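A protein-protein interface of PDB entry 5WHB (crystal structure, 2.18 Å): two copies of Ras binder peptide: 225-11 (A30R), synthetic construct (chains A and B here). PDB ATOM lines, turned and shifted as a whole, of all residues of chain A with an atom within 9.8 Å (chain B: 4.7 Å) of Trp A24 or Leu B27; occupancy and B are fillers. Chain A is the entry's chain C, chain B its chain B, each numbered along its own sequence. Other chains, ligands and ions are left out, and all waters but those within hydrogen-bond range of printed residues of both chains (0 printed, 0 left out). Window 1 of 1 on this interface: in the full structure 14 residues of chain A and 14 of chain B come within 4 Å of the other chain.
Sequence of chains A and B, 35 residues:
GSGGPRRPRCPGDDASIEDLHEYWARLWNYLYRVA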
ATOM      1  N   PRO A   8       7.387  30.888 -36.357  1.00  0.00           N
ATOM      2  CA  PRO A   8       6.082  30.295 -36.661  1.00  0.00           C
ATOM      3  C   PRO A   8       4.956  31.316 -36.565  1.00  0.00           C
ATOM      4  O   PRO A   8       5.086  32.322 -35.866  1.00  0.00           O
ATOM      5  CB  PRO A   8       5.931  29.214 -35.592  1.00  0.00           C
ATOM      6  CG  PRO A   8       6.751  29.704 -34.451  1.00  0.00           C
ATOM      7  CD  PRO A   8       7.926  30.408 -35.073  1.00  0.00           C
ATOM      8  N   ARG A   9       3.860  31.057 -37.266  1.00  0.00           N
ATOM      9  CA  ARG A   9       2.714  31.951 -37.222  1.00  0.00           C
ATOM     10  C   ARG A   9       1.638  31.401 -36.289  1.00  0.00           C
ATOM     11  O   ARG A   9       1.253  30.234 -36.387  1.00  0.00           O
ATOM     12  CB  ARG A   9       2.161  32.170 -38.631  1.00  0.00           C
ATOM     13  CG  ARG A   9       3.122  32.923 -39.552  1.00  0.00           C
ATOM     14  CD  ARG A   9       2.597  33.018 -40.984  1.00  0.00           C
ATOM     15  NE  ARG A   9       2.419  31.700 -41.589  1.00  0.00           N
ATOM     16  CZ  ARG A   9       1.973  31.495 -42.827  1.00  0.00           C
ATOM     17  NH1 ARG A   9       1.660  32.530 -43.595  1.00  0.00           N
ATOM     18  NH2 ARG A   9       1.842  30.258 -43.295  1.00  0.00           N
ATOM     19  N   CYS A  10       1.173  32.243 -35.370  1.00  0.00           N
ATOM     20  CA  CYS A  10       0.136  31.852 -34.422  1.00  0.00           C
ATOM     21  C   CYS A  10      -1.195  31.658 -35.139  1.00  0.00           C
ATOM     22  O   CYS A  10      -1.677  32.562 -35.826  1.00  0.00           O
ATOM     23  CB  CYS A  10      -0.007  32.897 -33.311  1.00  0.00           C
ATOM     24  SG  CYS A  10      -1.220  32.497 -32.031  1.00  0.00           S
ATOM     25  N   PRO A  11      -1.792  30.468 -34.983  1.00  0.00           N
ATOM     26  CA  PRO A  11      -3.068  30.110 -35.610  1.00  0.00           C
ATOM     27  C   PRO A  11      -4.237  30.910 -35.039  1.00  0.00           C
ATOM     28  O   PRO A  11      -4.154  31.389 -33.909  1.00  0.00           O
ATOM     29  CB  PRO A  11      -3.215  28.618 -35.283  1.00  0.00           C
ATOM     30  CG  PRO A  11      -1.844  28.157 -34.899  1.00  0.00           C
ATOM     31  CD  PRO A  11      -1.208  29.338 -34.244  1.00  0.00           C
ATOM     32  N   GLY A  12      -5.310  31.051 -35.813  1.00  0.00           N
ATOM     33  CA  GLY A  12      -6.461  31.832 -35.393  1.00  0.00           C
ATOM     34  C   GLY A  12      -7.358  31.127 -34.391  1.00  0.00           C
ATOM     35  O   GLY A  12      -6.949  30.166 -33.739  1.00  0.00           O
ATOM     36  N   SER A  16      -7.658  24.245 -34.349  1.00  0.00           N
ATOM     37  CA  SER A  16      -7.912  23.173 -33.397  1.00  0.00           C
ATOM     38  C   SER A  16      -6.821  23.119 -32.335  1.00  0.00           C
ATOM     39  O   SER A  16      -5.871  23.900 -32.368  1.00  0.00           O
ATOM     40  CB  SER A  16      -8.008  21.830 -34.121  1.00  0.00           C
ATOM     41  OG  SER A  16      -6.804  21.541 -34.813  1.00  0.00           O
ATOM     42  N   ILE A  17      -6.967  22.192 -31.394  1.00  0.00           N
ATOM     43  CA  ILE A  17      -5.974  21.996 -30.345  1.00  0.00           C
ATOM     44  C   ILE A  17      -4.653  21.524 -30.945  1.00  0.00           C
ATOM     45  O   ILE A  17      -3.576  21.942 -30.511  1.00  0.00           O
ATOM     46  CB  ILE A  17      -6.467  20.982 -29.290  1.00  0.00           C
ATOM     47  CG1 ILE A  17      -7.689  21.538 -28.558  1.00  0.00           C
ATOM     48  CG2 ILE A  17      -5.367  20.654 -28.292  1.00  0.00           C
ATOM     49  CD1 ILE A  17      -7.422  22.839 -27.831  1.00  0.00           C
ATOM     50  N   GLU A  18      -4.743  20.664 -31.955  1.00  0.00           N
ATOM     51  CA  GLU A  18      -3.561  20.159 -32.644  1.00  0.00           C
ATOM     52  C   GLU A  18      -2.787  21.297 -33.306  1.00  0.00           C
ATOM     53  O   GLU A  18      -1.557  21.292 -33.318  1.00  0.00           O
ATOM     54  CB  GLU A  18      -3.952  19.110 -33.688  1.00  0.00           C
ATOM     55  CG  GLU A  18      -2.765  18.429 -34.350  1.00  0.00           C
ATOM     56  CD  GLU A  18      -3.180  17.430 -35.414  1.00  0.00           C
ATOM     57  OE1 GLU A  18      -4.340  17.495 -35.874  1.00  0.00           O
ATOM     58  OE2 GLU A  18      -2.346  16.579 -35.788  1.00  0.00           O
ATOM     59  N   ASP A  19      -3.515  22.267 -33.850  1.00  0.00           N
ATOM     60  CA  ASP A  19      -2.901  23.443 -34.461  1.00  0.00           C
ATOM     61  C   ASP A  19      -2.071  24.218 -33.442  1.00  0.00           C
ATOM     62  O   ASP A  19      -0.979  24.696 -33.749  1.00  0.00           O
ATOM     63  CB  ASP A  19      -3.969  24.356 -35.066  1.00  0.00           C
ATOM     64  CG  ASP A  19      -4.647  23.743 -36.273  1.00  0.00           C
ATOM     65  OD1 ASP A  19      -3.982  22.982 -37.005  1.00  0.00           O
ATOM     66  OD2 ASP A  19      -5.844  24.022 -36.491  1.00  0.00           O
ATOM     67  N   LEU A  20      -2.602  24.340 -32.229  1.00  0.00           N
ATOM     68  CA  LEU A  20      -1.890  24.997 -31.141  1.00  0.00           C
ATOM     69  C   LEU A  20      -0.686  24.169 -30.714  1.00  0.00           C
ATOM     70  O   LEU A  20       0.354  24.711 -30.344  1.00  0.00           O
ATOM     71  CB  LEU A  20      -2.819  25.225 -29.950  1.00  0.00           C
ATOM     72  CG  LEU A  20      -4.026  26.129 -30.197  1.00  0.00           C
ATOM     73  CD1 LEU A  20      -4.951  26.112 -28.993  1.00  0.00           C
ATOM     74  CD2 LEU A  20      -3.573  27.546 -30.510  1.00  0.00           C
ATOM     75  N   HIS A  21      -0.840  22.848 -30.768  1.00  0.00           N
ATOM     76  CA  HIS A  21       0.235  21.926 -30.423  1.00  0.00           C
ATOM     77  C   HIS A  21       1.380  22.038 -31.421  1.00  0.00           C
ATOM     78  O   HIS A  21       2.551  22.010 -31.042  1.00  0.00           O
ATOM     79  CB  HIS A  21      -0.285  20.489 -30.376  1.00  0.00           C
ATOM     80  CG  HIS A  21       0.770  19.475 -30.059  1.00  0.00           C
ATOM     81  ND1 HIS A  21       1.200  19.223 -28.775  1.00  0.00           N
ATOM     82  CD2 HIS A  21       1.483  18.650 -30.863  1.00  0.00           C
ATOM     83  CE1 HIS A  21       2.131  18.287 -28.799  1.00  0.00           C
ATOM     84  NE2 HIS A  21       2.322  17.922 -30.055  1.00  0.00           N
ATOM     85  N   GLU A  22       1.031  22.161 -32.698  1.00  0.00           N
ATOM     86  CA  GLU A  22       2.021  22.351 -33.751  1.00  0.00           C
ATOM     87  C   GLU A  22       2.772  23.656 -33.539  1.00  0.00           C
ATOM     88  O   GLU A  22       4.001  23.686 -33.558  1.00  0.00           O
ATOM     89  CB  GLU A  22       1.353  22.344 -35.127  1.00  0.00           C
ATOM     90  CG  GLU A  22       0.715  21.017 -35.496  1.00  0.00           C
ATOM     91  CD  GLU A  22      -0.136  21.109 -36.745  1.00  0.00           C
ATOM     92  OE1 GLU A  22      -0.800  20.108 -37.088  1.00  0.00           O
ATOM     93  OE2 GLU A  22      -0.142  22.183 -37.385  1.00  0.00           O
ATOM     94  N   TYR A  23       2.022  24.733 -33.327  1.00  0.00           N
ATOM     95  CA  TYR A  23       2.611  26.041 -33.078  1.00  0.00           C
ATOM     96  C   TYR A  23       3.436  26.042 -31.793  1.00  0.00           C
ATOM     97  O   TYR A  23       4.446  26.737 -31.696  1.00  0.00           O
ATOM     98  CB  TYR A  23       1.522  27.113 -33.010  1.00  0.00           C
ATOM     99  CG  TYR A  23       2.040  28.482 -32.639  1.00  0.00           C
ATOM    100  CD1 TYR A  23       2.999  29.116 -33.418  1.00  0.00           C
ATOM    101  CD2 TYR A  23       1.569  29.142 -31.514  1.00  0.00           C
ATOM    102  CE1 TYR A  23       3.477  30.369 -33.081  1.00  0.00           C
ATOM    103  CE2 TYR A  23       2.039  30.394 -31.173  1.00  0.00           C
ATOM    104  CZ  TYR A  23       2.993  31.003 -31.958  1.00  0.00           C
ATOM    105  OH  TYR A  23       3.462  32.251 -31.617  1.00  0.00           O
ATOM    106  N   TRP A  24       3.002  25.255 -30.813  1.00  0.00           N
ATOM    107  CA  TRP A  24       3.736  25.103 -29.562  1.00  0.00           C
ATOM    108  C   TRP A  24       5.094  24.456 -29.806  1.00  0.00           C
ATOM    109  O   TRP A  24       6.108  24.889 -29.255  1.00  0.00           O
ATOM    110  CB  TRP A  24       2.923  24.272 -28.566  1.00  0.00           C
ATOM    111  CG  TRP A  24       3.671  23.890 -27.323  1.00  0.00           C
ATOM    112  CD1 TRP A  24       3.822  24.639 -26.192  1.00  0.00           C
ATOM    113  CD2 TRP A  24       4.363  22.657 -27.082  1.00  0.00           C
ATOM    114  NE1 TRP A  24       4.569  23.953 -25.265  1.00  0.00           N
ATOM    115  CE2 TRP A  24       4.913  22.734 -25.787  1.00  0.00           C
ATOM    116  CE3 TRP A  24       4.574  21.499 -27.837  1.00  0.00           C
ATOM    117  CZ2 TRP A  24       5.660  21.697 -25.229  1.00  0.00           C
ATOM    118  CZ3 TRP A  24       5.314  20.471 -27.283  1.00  0.00           C
ATOM    119  CH2 TRP A  24       5.848  20.576 -25.993  1.00  0.00           C
ATOM    120  N   ALA A  25       5.107  23.421 -30.640  1.00  0.00           N
ATOM    121  CA  ALA A  25       6.335  22.702 -30.958  1.00  0.00           C
ATOM    122  C   ALA A  25       7.269  23.545 -31.822  1.00  0.00           C
ATOM    123  O   ALA A  25       8.490  23.489 -31.669  1.00  0.00           O
ATOM    124  CB  ALA A  25       6.011  21.389 -31.657  1.00  0.00           C
ATOM    125  N   ARG A  26       6.689  24.327 -32.728  1.00  0.00           N
ATOM    126  CA  ARG A  26       7.472  25.186 -33.609  1.00  0.00           C
ATOM    127  C   ARG A  26       8.071  26.364 -32.849  1.00  0.00           C
ATOM    128  O   ARG A  26       9.222  26.740 -33.079  1.00  0.00           O
ATOM    129  CB  ARG A  26       6.611  25.695 -34.767  1.00  0.00           C
ATOM    130  CG  ARG A  26       6.097  24.602 -35.689  1.00  0.00           C
ATOM    131  CD  ARG A  26       5.181  25.170 -36.761  1.00  0.00           C
ATOM    132  NE  ARG A  26       4.489  24.118 -37.503  1.00  0.00           N
ATOM    133  CZ  ARG A  26       4.972  23.531 -38.592  1.00  0.00           C
ATOM    134  NH1 ARG A  26       6.153  23.891 -39.075  1.00  0.00           N
ATOM    135  NH2 ARG A  26       4.272  22.583 -39.201  1.00  0.00           N
ATOM    136  N   LEU A  27       7.287  26.944 -31.945  1.00  0.00           N
ATOM    137  CA  LEU A  27       7.736  28.091 -31.163  1.00  0.00           C
ATOM    138  C   LEU A  27       8.901  27.714 -30.255  1.00  0.00           C
ATOM    139  O   LEU A  27       9.889  28.444 -30.164  1.00  0.00           O
ATOM    140  CB  LEU A  27       6.585  28.661 -30.335  1.00  0.00           C
ATOM    141  CG  LEU A  27       6.869  29.964 -29.589  1.00  0.00           C
ATOM    142  CD1 LEU A  27       7.301  31.048 -30.562  1.00  0.00           C
ATOM    143  CD2 LEU A  27       5.646  30.404 -28.802  1.00  0.00           C
ATOM    144  N   TRP A  28       8.778  26.571 -29.588  1.00  0.00           N
ATOM    145  CA  TRP A  28       9.839  26.056 -28.731  1.00  0.00           C
ATOM    146  C   TRP A  28      11.121  25.841 -29.527  1.00  0.00           C
ATOM    147  O   TRP A  28      12.214  26.159 -29.060  1.00  0.00           O
ATOM    148  CB  TRP A  28       9.402  24.748 -28.066  1.00  0.00           C
ATOM    149  CG  TRP A  28      10.465  24.109 -27.224  1.00  0.00           C
ATOM    150  CD1 TRP A  28      10.700  24.321 -25.897  1.00  0.00           C
ATOM    151  CD2 TRP A  28      11.435  23.146 -27.653  1.00  0.00           C
ATOM    152  NE1 TRP A  28      11.758  23.554 -25.474  1.00  0.00           N
ATOM    153  CE2 TRP A  28      12.227  22.823 -26.533  1.00  0.00           C
ATOM    154  CE3 TRP A  28      11.714  22.528 -28.877  1.00  0.00           C
ATOM    155  CZ2 TRP A  28      13.276  21.909 -26.599  1.00  0.00           C
ATOM    156  CZ3 TRP A  28      12.756  21.620 -28.940  1.00  0.00           C
ATOM    157  CH2 TRP A  28      13.524  21.320 -27.809  1.00  0.00           C
ATOM    158  N   ASN A  29      10.977  25.302 -30.733  1.00  0.00           N
ATOM    159  CA  ASN A  29      12.119  25.064 -31.605  1.00  0.00           C
ATOM    160  C   ASN A  29      12.756  26.369 -32.067  1.00  0.00           C
ATOM    161  O   ASN A  29      13.977  26.474 -32.168  1.00  0.00           O
ATOM    162  CB  ASN A  29      11.701  24.228 -32.816  1.00  0.00           C
ATOM    163  CG  ASN A  29      12.872  23.874 -33.712  1.00  0.00           C
ATOM    164  OD1 ASN A  29      13.157  24.572 -34.686  1.00  0.00           O
ATOM    165  ND2 ASN A  29      13.557  22.784 -33.386  1.00  0.00           N
ATOM    166  N   TYR A  30      11.918  27.363 -32.343  1.00  0.00           N
ATOM    167  CA  TYR A  30      12.391  28.669 -32.788  1.00  0.00           C
ATOM    168  C   TYR A  30      13.130  29.406 -31.676  1.00  0.00           C
ATOM    169  O   TYR A  30      14.226  29.925 -31.887  1.00  0.00           O
ATOM    170  CB  TYR A  30      11.220  29.516 -33.293  1.00  0.00           C
ATOM    171  CG  TYR A  30      11.586  30.949 -33.610  1.00  0.00           C
ATOM    172  CD1 TYR A  30      12.215  31.278 -34.805  1.00  0.00           C
ATOM    173  CD2 TYR A  30      11.295  31.976 -32.720  1.00  0.00           C
ATOM    174  CE1 TYR A  30      12.549  32.587 -35.099  1.00  0.00           C
ATOM    175  CE2 TYR A  30      11.625  33.286 -33.008  1.00  0.00           C
ATOM    176  CZ  TYR A  30      12.251  33.586 -34.198  1.00  0.00           C
ATOM    177  OH  TYR A  30      12.580  34.891 -34.487  1.00  0.00           O
ATOM    178  N   LEU A  31      12.525  29.445 -30.493  1.00  0.00           N
ATOM    179  CA  LEU A  31      13.098  30.155 -29.353  1.00  0.00           C
ATOM    180  C   LEU A  31      14.420  29.536 -28.906  1.00  0.00           C
ATOM    181  O   LEU A  31      15.273  30.217 -28.338  1.00  0.00           O
ATOM    182  CB  LEU A  31      12.109  30.176 -28.184  1.00  0.00           C
ATOM    183  CG  LEU A  31      10.822  30.981 -28.377  1.00  0.00           C
ATOM    184  CD1 LEU A  31       9.909  30.834 -27.171  1.00  0.00           C
ATOM    185  CD2 LEU A  31      11.135  32.445 -28.638  1.00  0.00           C
ATOM    186  N   TYR A  32      14.585  28.244 -29.168  1.00  0.00           N
ATOM    187  CA  TYR A  32      15.800  27.534 -28.786  1.00  0.00           C
ATOM    188  C   TYR A  32      16.974  27.898 -29.691  1.00  0.00           C
ATOM    189  O   TYR A  32      18.097  28.083 -29.222  1.00  0.00           O
ATOM    190  CB  TYR A  32      15.566  26.020 -28.817  1.00  0.00           C
ATOM    191  CG  TYR A  32      16.819  25.199 -28.603  1.00  0.00           C
ATOM    192  CD1 TYR A  32      17.320  24.980 -27.326  1.00  0.00           C
ATOM    193  CD2 TYR A  32      17.499  24.639 -29.678  1.00  0.00           C
ATOM    194  CE1 TYR A  32      18.465  24.230 -27.127  1.00  0.00           C
ATOM    195  CE2 TYR A  32      18.644  23.889 -29.489  1.00  0.00           C
ATOM    196  CZ  TYR A  32      19.122  23.687 -28.211  1.00  0.00           C
ATOM    197  OH  TYR A  32      20.263  22.939 -28.018  1.00  0.00           O
ATOM    198  N   PRO B   8      -5.032  31.171 -24.287  1.00  0.00           N
ATOM    199  CA  PRO B   8      -4.186  32.369 -24.347  1.00  0.00           C
ATOM    200  C   PRO B   8      -4.207  33.034 -25.720  1.00  0.00           C
ATOM    201  O   PRO B   8      -4.043  32.358 -26.736  1.00  0.00           O
ATOM    202  CB  PRO B   8      -2.788  31.830 -24.020  1.00  0.00           C
ATOM    203  CG  PRO B   8      -2.855  30.373 -24.337  1.00  0.00           C
ATOM    204  CD  PRO B   8      -4.249  29.960 -23.990  1.00  0.00           C
ATOM    205  N   TYR B  23       4.215  33.762 -23.606  1.00  0.00           N
ATOM    206  CA  TYR B  23       3.066  33.112 -24.221  1.00  0.00           C
ATOM    207  C   TYR B  23       3.228  31.599 -24.233  1.00  0.00           C
ATOM    208  O   TYR B  23       2.296  30.863 -23.904  1.00  0.00           O
ATOM    209  CB  TYR B  23       2.856  33.622 -25.649  1.00  0.00           C
ATOM    210  CG  TYR B  23       1.819  32.836 -26.419  1.00  0.00           C
ATOM    211  CD1 TYR B  23       0.464  33.086 -26.251  1.00  0.00           C
ATOM    212  CD2 TYR B  23       2.195  31.840 -27.310  1.00  0.00           C
ATOM    213  CE1 TYR B  23      -0.484  32.367 -26.947  1.00  0.00           C
ATOM    214  CE2 TYR B  23       1.252  31.116 -28.009  1.00  0.00           C
ATOM    215  CZ  TYR B  23      -0.086  31.385 -27.827  1.00  0.00           C
ATOM    216  OH  TYR B  23      -1.032  30.668 -28.525  1.00  0.00           O
ATOM    217  N   TRP B  24       4.416  31.143 -24.620  1.00  0.00           N
ATOM    218  CA  TRP B  24       4.700  29.717 -24.730  1.00  0.00           C
ATOM    219  C   TRP B  24       4.478  28.996 -23.405  1.00  0.00           C
ATOM    220  O   TRP B  24       4.011  27.859 -23.382  1.00  0.00           O
ATOM    221  CB  TRP B  24       6.135  29.493 -25.214  1.00  0.00           C
ATOM    222  CG  TRP B  24       6.484  28.051 -25.415  1.00  0.00           C
ATOM    223  CD1 TRP B  24       6.423  27.348 -26.583  1.00  0.00           C
ATOM    224  CD2 TRP B  24       6.948  27.131 -24.417  1.00  0.00           C
ATOM    225  NE1 TRP B  24       6.820  26.049 -26.375  1.00  0.00           N
ATOM    226  CE2 TRP B  24       7.147  25.891 -25.053  1.00  0.00           C
ATOM    227  CE3 TRP B  24       7.213  27.238 -23.049  1.00  0.00           C
ATOM    228  CZ2 TRP B  24       7.600  24.766 -24.367  1.00  0.00           C
ATOM    229  CZ3 TRP B  24       7.662  26.121 -22.370  1.00  0.00           C
ATOM    230  CH2 TRP B  24       7.850  24.902 -23.029  1.00  0.00           C
ATOM    231  N   ALA B  25       4.816  29.664 -22.306  1.00  0.00           N
ATOM    232  CA  ALA B  25       4.657  29.086 -20.976  1.00  0.00           C
ATOM    233  C   ALA B  25       3.184  28.918 -20.613  1.00  0.00           C
ATOM    234  O   ALA B  25       2.800  27.932 -19.984  1.00  0.00           O
ATOM    235  CB  ALA B  25       5.364  29.946 -19.940  1.00  0.00           C
ATOM    236  N   ARG B  26       2.364  29.887 -21.011  1.00  0.00           N
ATOM    237  CA  ARG B  26       0.928  29.826 -20.764  1.00  0.00           C
ATOM    238  C   ARG B  26       0.261  28.822 -21.698  1.00  0.00           C
ATOM    239  O   ARG B  26      -0.678  28.128 -21.310  1.00  0.00           O
ATOM    240  CB  ARG B  26       0.298  31.213 -20.923  1.00  0.00           C
ATOM    241  CG  ARG B  26       0.646  32.167 -19.790  1.00  0.00           C
ATOM    242  CD  ARG B  26       0.945  33.570 -20.295  1.00  0.00           C
ATOM    243  NE  ARG B  26      -0.258  34.369 -20.496  1.00  0.00           N
ATOM    244  CZ  ARG B  26      -0.249  35.630 -20.919  1.00  0.00           C
ATOM    245  NH1 ARG B  26       0.903  36.230 -21.190  1.00  0.00           N
ATOM    246  NH2 ARG B  26      -1.389  36.290 -21.074  1.00  0.00           N
ATOM    247  N   LEU B  27       0.758  28.745 -22.929  1.00  0.00           N
ATOM    248  CA  LEU B  27       0.271  27.763 -23.889  1.00  0.00           C
ATOM    249  C   LEU B  27       0.649  26.358 -23.437  1.00  0.00           C
ATOM    250  O   LEU B  27      -0.093  25.402 -23.656  1.00  0.00           O
ATOM    251  CB  LEU B  27       0.836  28.045 -25.284  1.00  0.00           C
ATOM    252  CG  LEU B  27       0.386  27.113 -26.411  1.00  0.00           C
ATOM    253  CD1 LEU B  27      -1.128  27.126 -26.551  1.00  0.00           C
ATOM    254  CD2 LEU B  27       1.053  27.491 -27.726  1.00  0.00           C
ATOM    255  N   TRP B  28       1.811  26.250 -22.799  1.00  0.00           N
ATOM    256  CA  TRP B  28       2.310  24.981 -22.283  1.00  0.00           C
ATOM    257  C   TRP B  28       1.350  24.389 -21.256  1.00  0.00           C
ATOM    258  O   TRP B  28       1.047  23.196 -21.291  1.00  0.00           O
ATOM    259  CB  TRP B  28       3.695  25.173 -21.659  1.00  0.00           C
ATOM    260  CG  TRP B  28       4.423  23.898 -21.356  1.00  0.00           C
ATOM    261  CD1 TRP B  28       4.189  22.667 -21.896  1.00  0.00           C
ATOM    262  CD2 TRP B  28       5.508  23.730 -20.434  1.00  0.00           C
ATOM    263  NE1 TRP B  28       5.062  21.744 -21.370  1.00  0.00           N
ATOM    264  CE2 TRP B  28       5.881  22.373 -20.469  1.00  0.00           C
ATOM    265  CE3 TRP B  28       6.200  24.598 -19.582  1.00  0.00           C
ATOM    266  CZ2 TRP B  28       6.916  21.861 -19.686  1.00  0.00           C
ATOM    267  CZ3 TRP B  28       7.227  24.089 -18.805  1.00  0.00           C
ATOM    268  CH2 TRP B  28       7.574  22.734 -18.863  1.00  0.00           C
ATOM    269  N   ASN B  29       0.873  25.232 -20.346  1.00  0.00           N
ATOM    270  CA  ASN B  29      -0.045  24.797 -19.303  1.00  0.00           C
ATOM    271  C   ASN B  29      -1.459  24.582 -19.829  1.00  0.00           C
ATOM    272  O   ASN B  29      -2.178  23.702 -19.357  1.00  0.00           O
ATOM    273  CB  ASN B  29      -0.066  25.810 -18.156  1.00  0.00           C
ATOM    274  CG  ASN B  29       1.207  25.786 -17.336  1.00  0.00           C
ATOM    275  OD1 ASN B  29       1.288  25.101 -16.316  1.00  0.00           O
ATOM    276  ND2 ASN B  29       2.212  26.532 -17.780  1.00  0.00           N
ATOM    277  N   TYR B  30      -1.850  25.390 -20.809  1.00  0.00           N
ATOM    278  CA  TYR B  30      -3.175  25.280 -21.408  1.00  0.00           C
ATOM    279  C   TYR B  30      -3.330  23.971 -22.177  1.00  0.00           C
ATOM    280  O   TYR B  30      -4.329  23.268 -22.023  1.00  0.00           O
ATOM    281  CB  TYR B  30      -3.445  26.468 -22.334  1.00  0.00           C
ATOM    282  CG  TYR B  30      -4.720  26.339 -23.137  1.00  0.00           C
ATOM    283  CD1 TYR B  30      -5.957  26.590 -22.558  1.00  0.00           C
ATOM    284  CD2 TYR B  30      -4.686  25.968 -24.476  1.00  0.00           C
ATOM    285  CE1 TYR B  30      -7.126  26.473 -23.288  1.00  0.00           C
ATOM    286  CE2 TYR B  30      -5.849  25.847 -25.214  1.00  0.00           C
ATOM    287  CZ  TYR B  30      -7.066  26.101 -24.615  1.00  0.00           C
ATOM    288  OH  TYR B  30      -8.226  25.983 -25.348  1.00  0.00           O
ATOM    289  N   LEU B  31      -2.339  23.653 -23.002  1.00  0.00           N
ATOM    290  CA  LEU B  31      -2.373  22.445 -23.820  1.00  0.00           C
ATOM    291  C   LEU B  31      -2.367  21.181 -22.970  1.00  0.00           C
ATOM    292  O   LEU B  31      -2.984  20.179 -23.331  1.00  0.00           O
ATOM    293  CB  LEU B  31      -1.192  22.423 -24.791  1.00  0.00           C
ATOM    294  CG  LEU B  31      -1.275  23.384 -25.977  1.00  0.00           C
ATOM    295  CD1 LEU B  31      -0.050  23.236 -26.857  1.00  0.00           C
ATOM    296  CD2 LEU B  31      -2.544  23.136 -26.776  1.00  0.00           C
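The indole nitrogen (NE1) of Trp B24 is in hydrogen-bond range of the backbone carbonyl oxygen (O) of Trp A24 (3.2 Å).
Among the printed residues, merely in contact across the chains: Cys A10 with Tyr B23, Leu A20 with Leu B27, Leu A20 with Tyr B30, Leu A20 with Leu B31, His A21 with Leu B31, Tyr A23 with Tyr B23, Trp A24 with Leu B27, Trp A24 with Trp B28, Trp A24 with Leu B31, Leu A27 with Trp B24 and Trp A28 with Trp B24.
Of the printed residues of chain B, Trp A24 touches Trp B24, Leu B27, Trp B28 and Leu B31.
Leu B27 touches just these residues of chain A: Leu A20 and Trp A24.
Printed residues of chain A within 4 Å of Trp B28: Trp A24.
Printed residues of chain A within 4 Å of Leu B31: Leu A20 (3.8 Å), His A21 (3.8 Å) and Trp A24 (3.6 Å).
Of the printed residues of chain B, His A21 touches Leu B31 (3.8 Å).
Of the printed residues of chain A, Tyr B23 touches Cys A10 (3.96 Å) and Tyr A23 (3.3 Å).
Of the printed residues of chain A, Tyr B30 touches Leu A20 (3.9 Å).
Pro B8 touches none of the printed residues of chain A.
The nearest printed residue of chain B that does not touch Trp A24 is Asn B29 (6.3 Å).
The nearest residue of chain A that does not touch Leu B27 is Tyr A23 (4.2 Å).
Of the 22 printed residues of chain A, 7 touch a printed residue of chain B.
Printed residues of chain A that touch a printed residue of chain B: Cys A10, Leu A20, His A21, Tyr A23, Trp A24, Leu A27 and Trp A28.
Hydrophobic or aromatic side chains of chain A that line the printed part of chain B: Leu A20, Tyr A23, Trp A24, Leu A27 and Trp A28.
Tyr A23 touches its own counterpart, Tyr B23.
Trp A24 touches its own counterpart, Trp B24.
Trp A24 touches Leu B27, and with the chains exchanged Leu A27 touches Trp B24.
Trp A24 touches Leu B31, but with the chains exchanged Leu A31 does not touch Trp B24 (4.5 Å).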
